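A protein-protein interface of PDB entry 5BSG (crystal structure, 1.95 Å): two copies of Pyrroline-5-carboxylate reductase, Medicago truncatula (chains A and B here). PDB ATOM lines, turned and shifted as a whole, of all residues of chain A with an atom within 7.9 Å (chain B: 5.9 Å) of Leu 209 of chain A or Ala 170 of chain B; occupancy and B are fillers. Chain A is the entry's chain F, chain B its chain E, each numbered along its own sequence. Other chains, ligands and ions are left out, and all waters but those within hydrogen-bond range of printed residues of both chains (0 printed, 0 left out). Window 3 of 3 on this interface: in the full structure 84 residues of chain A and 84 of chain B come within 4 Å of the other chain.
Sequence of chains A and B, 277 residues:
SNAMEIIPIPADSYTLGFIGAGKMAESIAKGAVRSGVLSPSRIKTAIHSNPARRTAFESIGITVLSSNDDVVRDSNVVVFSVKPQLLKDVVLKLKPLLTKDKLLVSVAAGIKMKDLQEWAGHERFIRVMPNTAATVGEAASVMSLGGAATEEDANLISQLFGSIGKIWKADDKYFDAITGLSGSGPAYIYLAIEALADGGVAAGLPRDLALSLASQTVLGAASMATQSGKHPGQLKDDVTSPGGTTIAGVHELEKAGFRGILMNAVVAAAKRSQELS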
ATOM      1  N   ALA A 197     -19.036  12.492  -6.477  1.00  0.00           N
ATOM      2  CA  ALA A 197     -18.937  13.955  -6.687  1.00  0.00           C
ATOM      3  C   ALA A 197     -20.018  14.688  -5.825  1.00  0.00           C
ATOM      4  O   ALA A 197     -19.685  15.653  -5.154  1.00  0.00           O
ATOM      5  CB  ALA A 197     -19.119  14.296  -8.127  1.00  0.00           C
ATOM      6  N   GLY A 200     -18.832  14.657  -2.346  1.00  0.00           N
ATOM      7  CA  GLY A 200     -17.831  15.698  -2.145  1.00  0.00           C
ATOM      8  C   GLY A 200     -18.447  17.084  -1.938  1.00  0.00           C
ATOM      9  O   GLY A 200     -18.062  17.836  -1.030  1.00  0.00           O
ATOM     10  N   VAL A 201     -19.414  17.396  -2.753  1.00  0.00           N
ATOM     11  CA  VAL A 201     -20.094  18.713  -2.692  1.00  0.00           C
ATOM     12  C   VAL A 201     -20.876  18.800  -1.375  1.00  0.00           C
ATOM     13  O   VAL A 201     -20.836  19.839  -0.696  1.00  0.00           O
ATOM     14  CB  VAL A 201     -20.980  18.958  -3.894  1.00  0.00           C
ATOM     15  CG1 VAL A 201     -21.849  20.211  -3.770  1.00  0.00           C
ATOM     16  CG2 VAL A 201     -20.122  19.085  -5.156  1.00  0.00           C
ATOM     17  N   GLY A 204     -18.668  19.847   1.269  1.00  0.00           N
ATOM     18  CA  GLY A 204     -18.166  21.205   1.160  1.00  0.00           C
ATOM     19  C   GLY A 204     -17.276  21.487  -0.036  1.00  0.00           C
ATOM     20  O   GLY A 204     -16.759  22.597  -0.150  1.00  0.00           O
ATOM     21  N   LEU A 205     -17.068  20.510  -0.945  1.00  0.00           N
ATOM     22  CA  LEU A 205     -16.138  20.752  -2.054  1.00  0.00           C
ATOM     23  C   LEU A 205     -16.752  21.460  -3.187  1.00  0.00           C
ATOM     24  O   LEU A 205     -17.927  21.256  -3.479  1.00  0.00           O
ATOM     25  CB  LEU A 205     -15.597  19.463  -2.640  1.00  0.00           C
ATOM     26  CG  LEU A 205     -14.732  18.626  -1.782  1.00  0.00           C
ATOM     27  CD1 LEU A 205     -14.264  17.401  -2.551  1.00  0.00           C
ATOM     28  CD2 LEU A 205     -13.495  19.401  -1.330  1.00  0.00           C
ATOM     29  N   PRO A 206     -15.956  22.295  -3.895  1.00  0.00           N
ATOM     30  CA  PRO A 206     -16.409  22.825  -5.218  1.00  0.00           C
ATOM     31  C   PRO A 206     -16.751  21.682  -6.198  1.00  0.00           C
ATOM     32  O   PRO A 206     -16.083  20.663  -6.207  1.00  0.00           O
ATOM     33  CB  PRO A 206     -15.169  23.603  -5.755  1.00  0.00           C
ATOM     34  CG  PRO A 206     -14.417  23.971  -4.502  1.00  0.00           C
ATOM     35  CD  PRO A 206     -14.590  22.732  -3.582  1.00  0.00           C
ATOM     36  N   ARG A 207     -17.772  21.881  -7.001  1.00  0.00           N
ATOM     37  CA  ARG A 207     -18.254  20.866  -7.957  1.00  0.00           C
ATOM     38  C   ARG A 207     -17.195  20.419  -8.938  1.00  0.00           C
ATOM     39  O   ARG A 207     -17.028  19.232  -9.138  1.00  0.00           O
ATOM     40  CB  ARG A 207     -19.472  21.399  -8.638  1.00  0.00           C
ATOM     41  CG  ARG A 207     -19.982  20.560  -9.814  1.00  0.00           C
ATOM     42  CD  ARG A 207     -20.516  19.207  -9.374  1.00  0.00           C
ATOM     43  NE  ARG A 207     -21.679  19.299  -8.533  1.00  0.00           N
ATOM     44  CZ  ARG A 207     -22.302  18.238  -7.978  1.00  0.00           C
ATOM     45  NH1 ARG A 207     -21.909  17.011  -8.251  1.00  0.00           N
ATOM     46  NH2 ARG A 207     -23.337  18.424  -7.178  1.00  0.00           N
ATOM     47  N   ASP A 208     -16.460  21.322  -9.580  1.00  0.00           N
ATOM     48  CA  ASP A 208     -15.496  20.939 -10.607  1.00  0.00           C
ATOM     49  C   ASP A 208     -14.375  20.071 -10.042  1.00  0.00           C
ATOM     50  O   ASP A 208     -13.963  19.093 -10.665  1.00  0.00           O
ATOM     51  CB  ASP A 208     -14.908  22.183 -11.278  1.00  0.00           C
ATOM     52  CG  ASP A 208     -14.087  23.027 -10.323  1.00  0.00           C
ATOM     53  OD1 ASP A 208     -14.202  22.822  -9.097  1.00  0.00           O
ATOM     54  OD2 ASP A 208     -13.326  23.895 -10.799  1.00  0.00           O
ATOM     55  N   LEU A 209     -13.899  20.423  -8.851  1.00  0.00           N
ATOM     56  CA  LEU A 209     -12.925  19.599  -8.162  1.00  0.00           C
ATOM     57  C   LEU A 209     -13.519  18.260  -7.762  1.00  0.00           C
ATOM     58  O   LEU A 209     -12.870  17.237  -7.849  1.00  0.00           O
ATOM     59  CB  LEU A 209     -12.408  20.328  -6.924  1.00  0.00           C
ATOM     60  CG  LEU A 209     -11.356  19.582  -6.131  1.00  0.00           C
ATOM     61  CD1 LEU A 209     -10.077  19.336  -6.947  1.00  0.00           C
ATOM     62  CD2 LEU A 209     -10.972  20.347  -4.872  1.00  0.00           C
ATOM     63  N   ALA A 210     -14.726  18.283  -7.208  1.00  0.00           N
ATOM     64  CA  ALA A 210     -15.349  17.041  -6.718  1.00  0.00           C
ATOM     65  C   ALA A 210     -15.519  16.016  -7.820  1.00  0.00           C
ATOM     66  O   ALA A 210     -15.199  14.839  -7.658  1.00  0.00           O
ATOM     67  CB  ALA A 210     -16.711  17.339  -6.105  1.00  0.00           C
ATOM     68  N   LEU A 211     -15.956  16.483  -8.967  1.00  0.00           N
ATOM     69  CA  LEU A 211     -16.133  15.608 -10.114  1.00  0.00           C
ATOM     70  C   LEU A 211     -14.781  15.128 -10.701  1.00  0.00           C
ATOM     71  O   LEU A 211     -14.621  13.953 -10.953  1.00  0.00           O
ATOM     72  CB  LEU A 211     -17.007  16.290 -11.178  1.00  0.00           C
ATOM     73  CG  LEU A 211     -17.282  15.420 -12.392  1.00  0.00           C
ATOM     74  CD1 LEU A 211     -18.014  14.143 -12.017  1.00  0.00           C
ATOM     75  CD2 LEU A 211     -18.096  16.235 -13.405  1.00  0.00           C
ATOM     76  N   SER A 212     -13.781  16.037 -10.768  1.00  0.00           N
ATOM     77  CA  SER A 212     -12.445  15.629 -11.182  1.00  0.00           C
ATOM     78  C   SER A 212     -11.830  14.595 -10.267  1.00  0.00           C
ATOM     79  O   SER A 212     -11.280  13.605 -10.713  1.00  0.00           O
ATOM     80  CB  SER A 212     -11.476  16.844 -11.258  1.00  0.00           C
ATOM     81  OG  SER A 212     -11.959  17.748 -12.215  1.00  0.00           O
ATOM     82  N   LEU A 213     -12.004  14.799  -8.990  1.00  0.00           N
ATOM     83  CA  LEU A 213     -11.476  13.845  -8.036  1.00  0.00           C
ATOM     84  C   LEU A 213     -12.190  12.516  -8.123  1.00  0.00           C
ATOM     85  O   LEU A 213     -11.549  11.450  -8.001  1.00  0.00           O
ATOM     86  CB  LEU A 213     -11.534  14.406  -6.617  1.00  0.00           C
ATOM     87  CG  LEU A 213     -10.554  15.524  -6.261  1.00  0.00           C
ATOM     88  CD1 LEU A 213     -10.780  16.015  -4.843  1.00  0.00           C
ATOM     89  CD2 LEU A 213      -9.083  15.128  -6.442  1.00  0.00           C
ATOM     90  N   ALA A 214     -13.524  12.559  -8.231  1.00  0.00           N
ATOM     91  CA  ALA A 214     -14.311  11.278  -8.254  1.00  0.00           C
ATOM     92  C   ALA A 214     -13.857  10.425  -9.420  1.00  0.00           C
ATOM     93  O   ALA A 214     -13.555   9.256  -9.248  1.00  0.00           O
ATOM     94  CB  ALA A 214     -15.776  11.591  -8.394  1.00  0.00           C
ATOM     95  N   SER A 215     -13.765  11.041 -10.602  1.00  0.00           N
ATOM     96  CA  SER A 215     -13.380  10.270 -11.780  1.00  0.00           C
ATOM     97  C   SER A 215     -11.990   9.699 -11.641  1.00  0.00           C
ATOM     98  O   SER A 215     -11.757   8.504 -11.912  1.00  0.00           O
ATOM     99  CB  SER A 215     -13.458  11.133 -13.079  1.00  0.00           C
ATOM    100  OG  SER A 215     -14.795  11.506 -13.244  1.00  0.00           O
ATOM    101  N   GLN A 216     -11.057  10.507 -11.209  1.00  0.00           N
ATOM    102  CA  GLN A 216      -9.682  10.050 -11.145  1.00  0.00           C
ATOM    103  C   GLN A 216      -9.448   9.061  -9.979  1.00  0.00           C
ATOM    104  O   GLN A 216      -8.591   8.148 -10.065  1.00  0.00           O
ATOM    105  CB  GLN A 216      -8.710  11.231 -11.011  1.00  0.00           C
ATOM    106  CG  GLN A 216      -7.210  10.860 -10.912  1.00  0.00           C
ATOM    107  CD  GLN A 216      -6.715  10.259 -12.213  1.00  0.00           C
ATOM    108  OE1 GLN A 216      -7.221  10.534 -13.287  1.00  0.00           O
ATOM    109  NE2 GLN A 216      -5.799   9.329 -12.089  1.00  0.00           N
ATOM    110  N   VAL B 142      -4.160  16.731  -4.616  1.00  0.00           N
ATOM    111  CA  VAL B 142      -4.516  18.137  -4.499  1.00  0.00           C
ATOM    112  C   VAL B 142      -3.458  18.844  -3.662  1.00  0.00           C
ATOM    113  O   VAL B 142      -2.998  18.323  -2.672  1.00  0.00           O
ATOM    114  CB  VAL B 142      -5.903  18.330  -3.851  1.00  0.00           C
ATOM    115  CG1 VAL B 142      -6.351  19.773  -3.991  1.00  0.00           C
ATOM    116  CG2 VAL B 142      -6.932  17.490  -4.535  1.00  0.00           C
ATOM    117  N   MET B 143      -3.119  20.062  -4.094  1.00  0.00           N
ATOM    118  CA  MET B 143      -2.185  20.904  -3.336  1.00  0.00           C
ATOM    119  C   MET B 143      -2.840  22.175  -2.785  1.00  0.00           C
ATOM    120  O   MET B 143      -3.738  22.730  -3.415  1.00  0.00           O
ATOM    121  CB  MET B 143      -0.946  21.275  -4.191  1.00  0.00           C
ATOM    122  CG  MET B 143      -1.195  22.309  -5.251  1.00  0.00           C
ATOM    123  SD  MET B 143       0.415  22.855  -6.028  1.00  0.00           S
ATOM    124  CE  MET B 143       0.480  21.644  -7.210  1.00  0.00           C
ATOM    125  N   SER B 144      -2.327  22.638  -1.683  1.00  0.00           N
ATOM    126  CA  SER B 144      -2.688  23.971  -1.149  1.00  0.00           C
ATOM    127  C   SER B 144      -1.403  24.690  -0.817  1.00  0.00           C
ATOM    128  O   SER B 144      -0.379  24.076  -0.495  1.00  0.00           O
ATOM    129  CB  SER B 144      -3.584  23.935   0.073  1.00  0.00           C
ATOM    130  OG  SER B 144      -2.902  23.308   1.128  1.00  0.00           O
ATOM    131  N   LEU B 145      -1.473  26.007  -0.947  1.00  0.00           N
ATOM    132  CA  LEU B 145      -0.285  26.840  -0.856  1.00  0.00           C
ATOM    133  C   LEU B 145      -0.257  27.605   0.398  1.00  0.00           C
ATOM    134  O   LEU B 145      -1.241  28.217   0.780  1.00  0.00           O
ATOM    135  CB  LEU B 145      -0.263  27.858  -2.017  1.00  0.00           C
ATOM    136  CG  LEU B 145      -0.421  27.378  -3.434  1.00  0.00           C
ATOM    137  CD1 LEU B 145      -0.022  28.540  -4.393  1.00  0.00           C
ATOM    138  CD2 LEU B 145       0.425  26.195  -3.734  1.00  0.00           C
ATOM    139  N   TRP B 168      -4.472  18.850  -8.801  1.00  0.00           N
ATOM    140  CA  TRP B 168      -5.274  20.051  -8.811  1.00  0.00           C
ATOM    141  C   TRP B 168      -4.898  20.923  -7.551  1.00  0.00           C
ATOM    142  O   TRP B 168      -4.144  20.482  -6.699  1.00  0.00           O
ATOM    143  CB  TRP B 168      -6.742  19.709  -8.774  1.00  0.00           C
ATOM    144  CG  TRP B 168      -7.213  18.978  -9.970  1.00  0.00           C
ATOM    145  CD1 TRP B 168      -7.675  19.518 -11.106  1.00  0.00           C
ATOM    146  CD2 TRP B 168      -7.332  17.561 -10.123  1.00  0.00           C
ATOM    147  NE1 TRP B 168      -8.050  18.542 -12.008  1.00  0.00           N
ATOM    148  CE2 TRP B 168      -7.839  17.320 -11.427  1.00  0.00           C
ATOM    149  CE3 TRP B 168      -7.029  16.482  -9.307  1.00  0.00           C
ATOM    150  CZ2 TRP B 168      -8.051  16.028 -11.950  1.00  0.00           C
ATOM    151  CZ3 TRP B 168      -7.294  15.183  -9.797  1.00  0.00           C
ATOM    152  CH2 TRP B 168      -7.779  14.973 -11.118  1.00  0.00           C
ATOM    153  N   LYS B 169      -5.384  22.153  -7.541  1.00  0.00           N
ATOM    154  CA  LYS B 169      -5.120  23.096  -6.452  1.00  0.00           C
ATOM    155  C   LYS B 169      -6.373  23.432  -5.728  1.00  0.00           C
ATOM    156  O   LYS B 169      -7.381  23.567  -6.337  1.00  0.00           O
ATOM    157  CB  LYS B 169      -4.602  24.411  -6.998  1.00  0.00           C
ATOM    158  CG  LYS B 169      -3.304  24.224  -7.695  1.00  0.00           C
ATOM    159  CD  LYS B 169      -2.710  25.503  -8.267  1.00  0.00           C
ATOM    160  CE  LYS B 169      -1.446  25.114  -9.027  1.00  0.00           C
ATOM    161  NZ  LYS B 169      -1.019  26.241  -9.864  1.00  0.00           N
ATOM    162  N   ALA B 170      -6.318  23.533  -4.416  1.00  0.00           N
ATOM    163  CA  ALA B 170      -7.497  23.920  -3.657  1.00  0.00           C
ATOM    164  C   ALA B 170      -7.100  24.513  -2.344  1.00  0.00           C
ATOM    165  O   ALA B 170      -6.021  24.267  -1.828  1.00  0.00           O
ATOM    166  CB  ALA B 170      -8.398  22.754  -3.400  1.00  0.00           C
ATOM    167  N   ASP B 171      -8.007  25.303  -1.786  1.00  0.00           N
ATOM    168  CA  ASP B 171      -7.820  25.926  -0.492  1.00  0.00           C
ATOM    169  C   ASP B 171      -7.724  24.842   0.556  1.00  0.00           C
ATOM    170  O   ASP B 171      -8.417  23.815   0.466  1.00  0.00           O
ATOM    171  CB  ASP B 171      -9.027  26.816  -0.224  1.00  0.00           C
ATOM    172  CG  ASP B 171      -8.878  27.741   1.013  1.00  0.00           C
ATOM    173  OD1 ASP B 171      -8.671  27.307   2.163  1.00  0.00           O
ATOM    174  OD2 ASP B 171      -9.091  28.938   0.804  1.00  0.00           O
ATOM    175  N   ASP B 172      -6.892  25.096   1.566  1.00  0.00           N
ATOM    176  CA  ASP B 172      -6.672  24.161   2.638  1.00  0.00           C
ATOM    177  C   ASP B 172      -7.936  23.766   3.336  1.00  0.00           C
ATOM    178  O   ASP B 172      -8.068  22.661   3.802  1.00  0.00           O
ATOM    179  CB  ASP B 172      -5.703  24.720   3.658  1.00  0.00           C
ATOM    180  CG  ASP B 172      -4.958  23.606   4.443  1.00  0.00           C
ATOM    181  OD1 ASP B 172      -4.181  22.837   3.806  1.00  0.00           O
ATOM    182  OD2 ASP B 172      -5.063  23.556   5.666  1.00  0.00           O
ATOM    183  N   TYR B 174     -10.626  22.765   2.283  1.00  0.00           N
ATOM    184  CA  TYR B 174     -11.316  21.647   1.584  1.00  0.00           C
ATOM    185  C   TYR B 174     -10.724  20.299   1.878  1.00  0.00           C
ATOM    186  O   TYR B 174     -11.238  19.268   1.412  1.00  0.00           O
ATOM    187  CB  TYR B 174     -11.313  21.928   0.098  1.00  0.00           C
ATOM    188  CG  TYR B 174     -12.098  23.147  -0.344  1.00  0.00           C
ATOM    189  CD1 TYR B 174     -13.412  23.314   0.054  1.00  0.00           C
ATOM    190  CD2 TYR B 174     -11.542  24.134  -1.134  1.00  0.00           C
ATOM    191  CE1 TYR B 174     -14.144  24.399  -0.347  1.00  0.00           C
ATOM    192  CE2 TYR B 174     -12.225  25.253  -1.483  1.00  0.00           C
ATOM    193  CZ  TYR B 174     -13.525  25.384  -1.089  1.00  0.00           C
ATOM    194  OH  TYR B 174     -14.292  26.462  -1.479  1.00  0.00           O
ATOM    195  N   PHE B 175      -9.619  20.250   2.641  1.00  0.00           N
ATOM    196  CA  PHE B 175      -8.853  19.002   2.687  1.00  0.00           C
ATOM    197  C   PHE B 175      -9.476  17.851   3.509  1.00  0.00           C
ATOM    198  O   PHE B 175      -9.273  16.688   3.180  1.00  0.00           O
ATOM    199  CB  PHE B 175      -7.405  19.267   3.074  1.00  0.00           C
ATOM    200  CG  PHE B 175      -6.536  19.622   1.895  1.00  0.00           C
ATOM    201  CD1 PHE B 175      -6.853  20.723   1.124  1.00  0.00           C
ATOM    202  CD2 PHE B 175      -5.497  18.811   1.514  1.00  0.00           C
ATOM    203  CE1 PHE B 175      -6.069  21.067   0.029  1.00  0.00           C
ATOM    204  CE2 PHE B 175      -4.710  19.142   0.412  1.00  0.00           C
ATOM    205  CZ  PHE B 175      -5.018  20.245  -0.351  1.00  0.00           C
ATOM    206  N   ILE B 178     -11.664  16.432   0.786  1.00  0.00           N
ATOM    207  CA  ILE B 178     -10.785  15.769  -0.155  1.00  0.00           C
ATOM    208  C   ILE B 178     -10.397  14.362   0.398  1.00  0.00           C
ATOM    209  O   ILE B 178     -10.447  13.327  -0.340  1.00  0.00           O
ATOM    210  CB  ILE B 178      -9.577  16.640  -0.515  1.00  0.00           C
ATOM    211  CG1 ILE B 178     -10.053  17.820  -1.352  1.00  0.00           C
ATOM    212  CG2 ILE B 178      -8.506  15.868  -1.269  1.00  0.00           C
ATOM    213  CD1 ILE B 178      -9.049  18.972  -1.410  1.00  0.00           C
ATOM    214  N   LEU B 181     -13.061  11.853  -0.014  1.00  0.00           N
ATOM    215  CA  LEU B 181     -13.365  11.497  -1.397  1.00  0.00           C
ATOM    216  C   LEU B 181     -12.185  10.821  -2.084  1.00  0.00           C
ATOM    217  O   LEU B 181     -12.204   9.633  -2.375  1.00  0.00           O
ATOM    218  CB  LEU B 181     -13.817  12.744  -2.109  1.00  0.00           C
ATOM    219  CG  LEU B 181     -14.081  12.613  -3.592  1.00  0.00           C
ATOM    220  CD1 LEU B 181     -15.001  11.468  -3.902  1.00  0.00           C
ATOM    221  CD2 LEU B 181     -14.656  13.876  -4.193  1.00  0.00           C
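The backbone NH of Met 143 of chain B is in hydrogen-bond range of the backbone carbonyl oxygen of Trp 168 of chain B, 2.8 Å away. The backbone carbonyl oxygen of Met 143 of chain B lies within hydrogen-bond range of the backbone NH of Ala 170 of chain B, at 2.9 Å. N of Leu 205 of chain A lies within hydrogen-bond range of O of Gly 200 of chain A, 2.9 Å away. The backbone carbonyl oxygen of Asp 208 of chain A sits at hydrogen-bond distance from the side-chain hydroxyl of Ser 212 of chain A, 2.9 Å away.
No position is printed for both chains.
Among the printed residues, merely in contact across the chains: Gly 204 of chain A with Tyr 174 of chain B, Leu 205 of chain A with Tyr 174 of chain B, Ser 212 of chain A with Trp 168 of chain B, Ala 210 of chain A with Leu 181 of chain B, Pro 206 of chain A with Tyr 174 of chain B, Leu 213 of chain A with Val 142 of chain B, Leu 213 of chain A with Trp 168 of chain B, Leu 205 of chain A with Ile 178 of chain B, Leu 209 of chain A with Ala 170 of chain B, Leu 209 of chain A with Trp 168 of chain B, Gln 216 of chain A with Trp 168 of chain B, Leu 205 of chain A with Leu 181 of chain B, Leu 213 of chain A with Leu 181 of chain B and Leu 213 of chain A with Ile 178 of chain B.
Of the 16 printed residues of chain A, 8 touch a printed residue of chain B. Hydrophobic or aromatic side chains of chain A within 4 Å of the printed part of chain B: Leu 205, Pro 206, Leu 209 and Leu 213. Printed residues of chain B that touch a printed residue of chain A: Val 142, Trp 168, Ala 170, Tyr 174, Ile 178 and Leu 181. Hydrophobic or aromatic side chains of chain B that line the printed part of chain A: Val 142, Trp 168, Ala 170, Tyr 174, Ile 178 and Leu 181. Among the printed residues, 14 pairs touch across the chains. Among the printed residues, no Asp or Glu carboxylate lies within 4 Å of a Lys or Arg side-chain nitrogen of the other chain.
Ala 170 of chain B touches one residue of chain A. Of the printed residues of chain A, Val 142 of chain B touches Leu 213. Printed residues of chain B within 4 Å of Gly 204 of chain A: Tyr 174 (3.2 Å). Printed residues of chain B within 4 Å of Gln 216 of chain A: Trp 168. Printed residues of chain A within 4 Å of Ile 178 of chain B: Leu 205 (3.8 Å) and Leu 213 (3.997 Å). Printed residues of chain A within 4 Å of Tyr 174 of chain B: Gly 204, Leu 205 and Pro 206. Ala 214 of chain A touches none of the printed residues of chain B. Ser 215 of chain A touches none of the printed residues of chain B. The nearest residue of chain B that does not touch Leu 209 of chain A is Ile 178 of chain B (4.2 Å). The nearest residue of chain A that does not touch Ala 170 of chain B is Pro 206 of chain A (6.2 Å). The nearest printed residue of chain B that does not touch Leu 213 of chain A is Tyr 174 of chain B (7.1 Å).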
